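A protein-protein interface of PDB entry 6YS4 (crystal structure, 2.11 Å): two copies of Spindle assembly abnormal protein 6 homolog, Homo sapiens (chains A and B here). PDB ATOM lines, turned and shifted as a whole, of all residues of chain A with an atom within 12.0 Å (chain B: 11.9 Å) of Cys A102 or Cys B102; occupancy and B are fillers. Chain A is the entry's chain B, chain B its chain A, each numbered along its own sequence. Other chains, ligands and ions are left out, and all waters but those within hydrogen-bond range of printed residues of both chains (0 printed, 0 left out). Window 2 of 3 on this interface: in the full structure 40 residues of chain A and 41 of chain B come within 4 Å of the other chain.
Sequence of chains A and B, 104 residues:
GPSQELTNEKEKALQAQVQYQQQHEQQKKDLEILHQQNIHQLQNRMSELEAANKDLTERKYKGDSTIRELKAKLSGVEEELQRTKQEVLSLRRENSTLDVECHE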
ATOM      1  N   ARG A  93      30.927 -18.852 -30.332  1.00  0.00           N
ATOM      2  CA  ARG A  93      31.851 -18.044 -31.123  1.00  0.00           C
ATOM      3  C   ARG A  93      31.615 -16.572 -30.833  1.00  0.00           C
ATOM      4  O   ARG A  93      32.570 -15.850 -30.565  1.00  0.00           O
ATOM      5  CB  ARG A  93      31.710 -18.342 -32.615  1.00  0.00           C
ATOM      6  CG  ARG A  93      32.441 -19.615 -33.012  1.00  0.00           C
ATOM      7  CD  ARG A  93      32.575 -19.792 -34.512  1.00  0.00           C
ATOM      8  NE  ARG A  93      31.286 -19.921 -35.206  1.00  0.00           N
ATOM      9  CZ  ARG A  93      30.665 -21.072 -35.474  1.00  0.00           C
ATOM     10  NH1 ARG A  93      31.199 -22.230 -35.099  1.00  0.00           N
ATOM     11  NH2 ARG A  93      29.516 -21.072 -36.130  1.00  0.00           N
ATOM     12  N   GLU A  94      30.329 -16.150 -30.810  1.00  0.00           N
ATOM     13  CA  GLU A  94      29.892 -14.784 -30.492  1.00  0.00           C
ATOM     14  C   GLU A  94      30.315 -14.420 -29.072  1.00  0.00           C
ATOM     15  O   GLU A  94      30.766 -13.310 -28.840  1.00  0.00           O
ATOM     16  CB  GLU A  94      28.367 -14.662 -30.608  1.00  0.00           C
ATOM     17  CG  GLU A  94      27.864 -14.409 -32.015  1.00  0.00           C
ATOM     18  CD  GLU A  94      26.365 -14.180 -32.120  1.00  0.00           C
ATOM     19  OE1 GLU A  94      25.665 -15.064 -32.667  1.00  0.00           O
ATOM     20  OE2 GLU A  94      25.889 -13.121 -31.646  1.00  0.00           O
ATOM     21  N   ASN A  95      30.153 -15.374 -28.133  1.00  0.00           N
ATOM     22  CA  ASN A  95      30.511 -15.278 -26.717  1.00  0.00           C
ATOM     23  C   ASN A  95      32.022 -15.126 -26.521  1.00  0.00           C
ATOM     24  O   ASN A  95      32.425 -14.404 -25.615  1.00  0.00           O
ATOM     25  CB  ASN A  95      30.001 -16.504 -25.959  1.00  0.00           C
ATOM     26  CG  ASN A  95      30.175 -16.431 -24.471  1.00  0.00           C
ATOM     27  OD1 ASN A  95      29.299 -15.957 -23.740  1.00  0.00           O
ATOM     28  ND2 ASN A  95      31.307 -16.913 -23.992  1.00  0.00           N
ATOM     29  N   SER A  96      32.849 -15.806 -27.349  1.00  0.00           N
ATOM     30  CA  SER A  96      34.313 -15.721 -27.294  1.00  0.00           C
ATOM     31  C   SER A  96      34.817 -14.367 -27.778  1.00  0.00           C
ATOM     32  O   SER A  96      35.717 -13.805 -27.149  1.00  0.00           O
ATOM     33  CB  SER A  96      34.965 -16.850 -28.081  1.00  0.00           C
ATOM     34  OG  SER A  96      34.634 -18.105 -27.512  1.00  0.00           O
ATOM     35  N   THR A  97      34.242 -13.845 -28.881  1.00  0.00           N
ATOM     36  CA  THR A  97      34.607 -12.548 -29.463  1.00  0.00           C
ATOM     37  C   THR A  97      34.217 -11.396 -28.525  1.00  0.00           C
ATOM     38  O   THR A  97      34.971 -10.432 -28.400  1.00  0.00           O
ATOM     39  CB  THR A  97      34.009 -12.370 -30.875  1.00  0.00           C
ATOM     40  OG1 THR A  97      32.591 -12.421 -30.799  1.00  0.00           O
ATOM     41  CG2 THR A  97      34.524 -13.396 -31.880  1.00  0.00           C
ATOM     42  N   LEU A  98      33.040 -11.495 -27.871  1.00  0.00           N
ATOM     43  CA  LEU A  98      32.578 -10.481 -26.918  1.00  0.00           C
ATOM     44  C   LEU A  98      33.440 -10.524 -25.648  1.00  0.00           C
ATOM     45  O   LEU A  98      33.824  -9.474 -25.148  1.00  0.00           O
ATOM     46  CB  LEU A  98      31.088 -10.666 -26.566  1.00  0.00           C
ATOM     47  CG  LEU A  98      30.047 -10.188 -27.590  1.00  0.00           C
ATOM     48  CD1 LEU A  98      28.693 -10.783 -27.291  1.00  0.00           C
ATOM     49  CD2 LEU A  98      29.926  -8.673 -27.611  1.00  0.00           C
ATOM     50  N   ASP A  99      33.767 -11.748 -25.156  1.00  0.00           N
ATOM     51  CA  ASP A  99      34.598 -11.984 -23.968  1.00  0.00           C
ATOM     52  C   ASP A  99      36.007 -11.407 -24.102  1.00  0.00           C
ATOM     53  O   ASP A  99      36.529 -10.894 -23.107  1.00  0.00           O
ATOM     54  CB  ASP A  99      34.649 -13.486 -23.610  1.00  0.00           C
ATOM     55  CG  ASP A  99      35.341 -13.846 -22.303  1.00  0.00           C
ATOM     56  OD1 ASP A  99      35.293 -13.030 -21.358  1.00  0.00           O
ATOM     57  OD2 ASP A  99      35.914 -14.954 -22.222  1.00  0.00           O
ATOM     58  N   VAL A 100      36.616 -11.461 -25.315  1.00  0.00           N
ATOM     59  CA  VAL A 100      37.963 -10.909 -25.552  1.00  0.00           C
ATOM     60  C   VAL A 100      37.946  -9.367 -25.538  1.00  0.00           C
ATOM     61  O   VAL A 100      38.888  -8.759 -25.013  1.00  0.00           O
ATOM     62  CB  VAL A 100      38.730 -11.482 -26.779  1.00  0.00           C
ATOM     63  CG1 VAL A 100      38.991 -12.977 -26.625  1.00  0.00           C
ATOM     64  CG2 VAL A 100      38.043 -11.173 -28.106  1.00  0.00           C
ATOM     65  N   GLU A 101      36.869  -8.745 -26.071  1.00  0.00           N
ATOM     66  CA  GLU A 101      36.703  -7.284 -26.071  1.00  0.00           C
ATOM     67  C   GLU A 101      36.482  -6.768 -24.636  1.00  0.00           C
ATOM     68  O   GLU A 101      36.967  -5.688 -24.287  1.00  0.00           O
ATOM     69  CB  GLU A 101      35.546  -6.864 -26.992  1.00  0.00           C
ATOM     70  CG  GLU A 101      35.868  -6.992 -28.473  1.00  0.00           C
ATOM     71  CD  GLU A 101      34.742  -6.655 -29.437  1.00  0.00           C
ATOM     72  OE1 GLU A 101      34.595  -7.382 -30.448  1.00  0.00           O
ATOM     73  OE2 GLU A 101      34.013  -5.663 -29.193  1.00  0.00           O
ATOM     74  N   CYS A 102      35.781  -7.577 -23.808  1.00  0.00           N
ATOM     75  CA  CYS A 102      35.457  -7.313 -22.407  1.00  0.00           C
ATOM     76  C   CYS A 102      36.614  -7.626 -21.476  1.00  0.00           C
ATOM     77  O   CYS A 102      37.377  -6.720 -21.147  1.00  0.00           O
ATOM     78  CB  CYS A 102      34.194  -8.059 -21.984  1.00  0.00           C
ATOM     79  SG  CYS A 102      32.667  -7.341 -22.629  1.00  0.00           S
ATOM     80  N   HIS A 103      36.720  -8.897 -21.023  1.00  0.00           N
ATOM     81  CA  HIS A 103      37.750  -9.371 -20.097  1.00  0.00           C
ATOM     82  C   HIS A 103      39.006  -9.776 -20.861  1.00  0.00           C
ATOM     83  O   HIS A 103      39.986  -9.036 -20.869  1.00  0.00           O
ATOM     84  CB  HIS A 103      37.237 -10.556 -19.254  1.00  0.00           C
ATOM     85  CG  HIS A 103      35.848 -10.386 -18.705  1.00  0.00           C
ATOM     86  ND1 HIS A 103      35.582  -9.509 -17.668  1.00  0.00           N
ATOM     87  CD2 HIS A 103      34.700 -11.012 -19.051  1.00  0.00           C
ATOM     88  CE1 HIS A 103      34.286  -9.621 -17.427  1.00  0.00           C
ATOM     89  NE2 HIS A 103      33.713 -10.511 -18.236  1.00  0.00           N
ATOM     90  N   ARG B  93      21.683 -15.004 -23.115  1.00  0.00           N
ATOM     91  CA  ARG B  93      21.648 -14.220 -21.885  1.00  0.00           C
ATOM     92  C   ARG B  93      23.022 -13.619 -21.610  1.00  0.00           C
ATOM     93  O   ARG B  93      23.095 -12.432 -21.286  1.00  0.00           O
ATOM     94  CB  ARG B  93      21.201 -15.123 -20.724  1.00  0.00           C
ATOM     95  CG  ARG B  93      20.681 -14.393 -19.497  1.00  0.00           C
ATOM     96  CD  ARG B  93      20.209 -15.364 -18.425  1.00  0.00           C
ATOM     97  NE  ARG B  93      19.093 -16.179 -18.892  1.00  0.00           N
ATOM     98  CZ  ARG B  93      19.093 -17.508 -18.952  1.00  0.00           C
ATOM     99  NH1 ARG B  93      20.153 -18.195 -18.535  1.00  0.00           N
ATOM    100  NH2 ARG B  93      18.041 -18.159 -19.414  1.00  0.00           N
ATOM    101  N   GLU B  94      24.100 -14.429 -21.777  1.00  0.00           N
ATOM    102  CA  GLU B  94      25.507 -14.060 -21.595  1.00  0.00           C
ATOM    103  C   GLU B  94      25.941 -13.058 -22.650  1.00  0.00           C
ATOM    104  O   GLU B  94      26.674 -12.124 -22.341  1.00  0.00           O
ATOM    105  CB  GLU B  94      26.415 -15.301 -21.710  1.00  0.00           C
ATOM    106  CG  GLU B  94      26.601 -16.100 -20.430  1.00  0.00           C
ATOM    107  CD  GLU B  94      27.652 -17.197 -20.532  1.00  0.00           C
ATOM    108  OE1 GLU B  94      27.276 -18.387 -20.647  1.00  0.00           O
ATOM    109  OE2 GLU B  94      28.858 -16.863 -20.483  1.00  0.00           O
ATOM    110  N   ASN B  95      25.537 -13.298 -23.903  1.00  0.00           N
ATOM    111  CA  ASN B  95      25.871 -12.460 -25.041  1.00  0.00           C
ATOM    112  C   ASN B  95      25.261 -11.094 -24.910  1.00  0.00           C
ATOM    113  O   ASN B  95      25.956 -10.129 -25.194  1.00  0.00           O
ATOM    114  CB  ASN B  95      25.488 -13.112 -26.365  1.00  0.00           C
ATOM    115  CG  ASN B  95      26.452 -14.189 -26.794  1.00  0.00           C
ATOM    116  OD1 ASN B  95      27.378 -14.558 -26.069  1.00  0.00           O
ATOM    117  ND2 ASN B  95      26.239 -14.735 -27.985  1.00  0.00           N
ATOM    118  N   SER B  96      24.000 -11.005 -24.431  1.00  0.00           N
ATOM    119  CA  SER B  96      23.290  -9.739 -24.240  1.00  0.00           C
ATOM    120  C   SER B  96      23.965  -8.846 -23.197  1.00  0.00           C
ATOM    121  O   SER B  96      24.118  -7.644 -23.438  1.00  0.00           O
ATOM    122  CB  SER B  96      21.831  -9.989 -23.873  1.00  0.00           C
ATOM    123  OG  SER B  96      21.161 -10.673 -24.919  1.00  0.00           O
ATOM    124  N   THR B  97      24.386  -9.445 -22.056  1.00  0.00           N
ATOM    125  CA  THR B  97      25.065  -8.753 -20.957  1.00  0.00           C
ATOM    126  C   THR B  97      26.440  -8.260 -21.390  1.00  0.00           C
ATOM    127  O   THR B  97      26.833  -7.152 -21.014  1.00  0.00           O
ATOM    128  CB  THR B  97      25.140  -9.625 -19.688  1.00  0.00           C
ATOM    129  OG1 THR B  97      25.866 -10.824 -19.956  1.00  0.00           O
ATOM    130  CG2 THR B  97      23.772  -9.949 -19.115  1.00  0.00           C
ATOM    131  N   LEU B  98      27.173  -9.078 -22.181  1.00  0.00           N
ATOM    132  CA  LEU B  98      28.498  -8.696 -22.685  1.00  0.00           C
ATOM    133  C   LEU B  98      28.368  -7.571 -23.720  1.00  0.00           C
ATOM    134  O   LEU B  98      29.141  -6.619 -23.671  1.00  0.00           O
ATOM    135  CB  LEU B  98      29.257  -9.895 -23.293  1.00  0.00           C
ATOM    136  CG  LEU B  98      29.873 -10.921 -22.333  1.00  0.00           C
ATOM    137  CD1 LEU B  98      30.220 -12.186 -23.065  1.00  0.00           C
ATOM    138  CD2 LEU B  98      31.121 -10.384 -21.646  1.00  0.00           C
ATOM    139  N   ASP B  99      27.363  -7.669 -24.620  1.00  0.00           N
ATOM    140  CA  ASP B  99      27.076  -6.696 -25.675  1.00  0.00           C
ATOM    141  C   ASP B  99      26.738  -5.312 -25.129  1.00  0.00           C
ATOM    142  O   ASP B  99      27.162  -4.323 -25.728  1.00  0.00           O
ATOM    143  CB  ASP B  99      25.966  -7.200 -26.614  1.00  0.00           C
ATOM    144  CG  ASP B  99      25.681  -6.365 -27.853  1.00  0.00           C
ATOM    145  OD1 ASP B  99      26.624  -5.710 -28.367  1.00  0.00           O
ATOM    146  OD2 ASP B  99      24.525  -6.390 -28.330  1.00  0.00           O
ATOM    147  N   VAL B 100      26.001  -5.231 -23.991  1.00  0.00           N
ATOM    148  CA  VAL B 100      25.645  -3.938 -23.383  1.00  0.00           C
ATOM    149  C   VAL B 100      26.887  -3.238 -22.776  1.00  0.00           C
ATOM    150  O   VAL B 100      26.973  -2.017 -22.847  1.00  0.00           O
ATOM    151  CB  VAL B 100      24.434  -3.966 -22.404  1.00  0.00           C
ATOM    152  CG1 VAL B 100      23.151  -4.377 -23.123  1.00  0.00           C
ATOM    153  CG2 VAL B 100      24.682  -4.834 -21.174  1.00  0.00           C
ATOM    154  N   GLU B 101      27.873  -4.021 -22.290  1.00  0.00           N
ATOM    155  CA  GLU B 101      29.124  -3.549 -21.685  1.00  0.00           C
ATOM    156  C   GLU B 101      30.165  -3.035 -22.703  1.00  0.00           C
ATOM    157  O   GLU B 101      31.091  -2.329 -22.308  1.00  0.00           O
ATOM    158  CB  GLU B 101      29.720  -4.632 -20.774  1.00  0.00           C
ATOM    159  CG  GLU B 101      28.878  -4.887 -19.534  1.00  0.00           C
ATOM    160  CD  GLU B 101      29.245  -6.081 -18.674  1.00  0.00           C
ATOM    161  OE1 GLU B 101      28.515  -6.340 -17.688  1.00  0.00           O
ATOM    162  OE2 GLU B 101      30.256  -6.757 -18.976  1.00  0.00           O
ATOM    163  N   CYS B 102      30.019  -3.389 -23.997  1.00  0.00           N
ATOM    164  CA  CYS B 102      30.908  -2.940 -25.082  1.00  0.00           C
ATOM    165  C   CYS B 102      30.264  -1.780 -25.812  1.00  0.00           C
ATOM    166  O   CYS B 102      30.968  -0.876 -26.270  1.00  0.00           O
ATOM    167  CB  CYS B 102      31.210  -4.069 -26.066  1.00  0.00           C
ATOM    168  SG  CYS B 102      31.980  -5.529 -25.339  1.00  0.00           S
ATOM    169  N   HIS B 103      28.931  -1.858 -25.987  1.00  0.00           N
ATOM    170  CA  HIS B 103      28.110  -0.925 -26.744  1.00  0.00           C
ATOM    171  C   HIS B 103      27.249  -0.102 -25.792  1.00  0.00           C
ATOM    172  O   HIS B 103      27.091   1.099 -25.989  1.00  0.00           O
ATOM    173  CB  HIS B 103      27.212  -1.705 -27.738  1.00  0.00           C
ATOM    174  CG  HIS B 103      27.921  -2.676 -28.656  1.00  0.00           C
ATOM    175  ND1 HIS B 103      28.910  -3.537 -28.198  1.00  0.00           N
ATOM    176  CD2 HIS B 103      27.681  -2.957 -29.958  1.00  0.00           C
ATOM    177  CE1 HIS B 103      29.283  -4.256 -29.243  1.00  0.00           C
ATOM    178  NE2 HIS B 103      28.561  -3.956 -30.321  1.00  0.00           N
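SG of Cys A102 is in hydrogen-bond range of SG of Cys B102 (3.3 Å). OE2 of Glu B94 lies close to OD1 of Asn A95 (3.4 Å). SG of Cys A102 lies close to O of Leu B98. OD1 of Asn B95 lies close to OD1 of Asn A95.
The backbone carbonyl oxygen of Glu B94 sits at hydrogen-bond distance from the side-chain hydroxyl of Thr B97, at 2.8 Å. A ring nitrogen (ND1) of His B103 sits at hydrogen-bond distance from the backbone carbonyl oxygen of Asp B99, 3.1 Å away. The backbone carbonyl oxygen (O) of Leu B98 is in hydrogen-bond range of the side-chain sulfur (SG) of Cys B102. The backbone carbonyl oxygen (O) of Glu A94 is in hydrogen-bond range of the side-chain hydroxyl (OG1) of Thr A97 (2.8 Å). SG of Cys A102 lies close to O of Leu A98 (3.5 Å).
Among the printed residues, merely in contact across the chains: Glu A94 with Asn B95 (3.4 Å), Leu A98 with Asn B95 (3.5 Å), Leu A98 with Leu B98 (3.8 Å), Asn A95 with Leu B98 (3.9 Å) and Leu A98 with Asp B99 (3.97 Å).
Printed residues of chain B within 4 Å of Glu A94: Asn B95. Of the printed residues of chain B, Asn A95 touches Glu B94 (3.4 Å), Asn B95 (3.3 Å) and Leu B98 (3.9 Å). Leu A98 touches three residues of chain B. No residue of chain B comes within 4 Å of Asp A99. No residue of chain B comes within 4 Å of Glu A101. Cys A102 touches just these residues of chain B: Leu B98 and Cys B102. No residue of chain B comes within 4 Å of His A103. Of the printed residues of chain A, Glu B94 touches Asn A95. Printed residues of chain A within 4 Å of Asn B95: Glu A94 (3.4 Å), Asn A95 (3.3 Å) and Leu A98 (3.5 Å). Of chain A, only Asn A95, Leu A98 and Cys A102 come within 4 Å of Leu B98. Asp B99 touches just one residue of chain A: Leu A98. No residue of chain A comes within 4 Å of Glu B101. Cys B102 touches just one residue of chain A: Cys A102 (3.3 Å). No residue of chain A comes within 4 Å of His B103. The nearest residue of chain B that does not touch Cys A102 is Glu B101 (4.4 Å). The nearest printed residue of chain B that does not touch Asn A95 is Arg B93 (7.0 Å).
Hydrophobic or aromatic side chains of chain B that line the printed part of chain A: Leu B98. Among the printed residues, no Asp or Glu carboxylate lies within 4 Å of a Lys or Arg side-chain nitrogen of the other chain.
Glu A94 touches Asn B95, and with the chains exchanged Asn A95 touches Glu B94. Asn B95 touches its own counterpart, Asn A95. Asn A95 touches Leu B98, and with the chains exchanged Leu A98 touches Asn B95. Cys B102 touches its own counterpart, Cys A102. 11 positions are printed for both chains.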
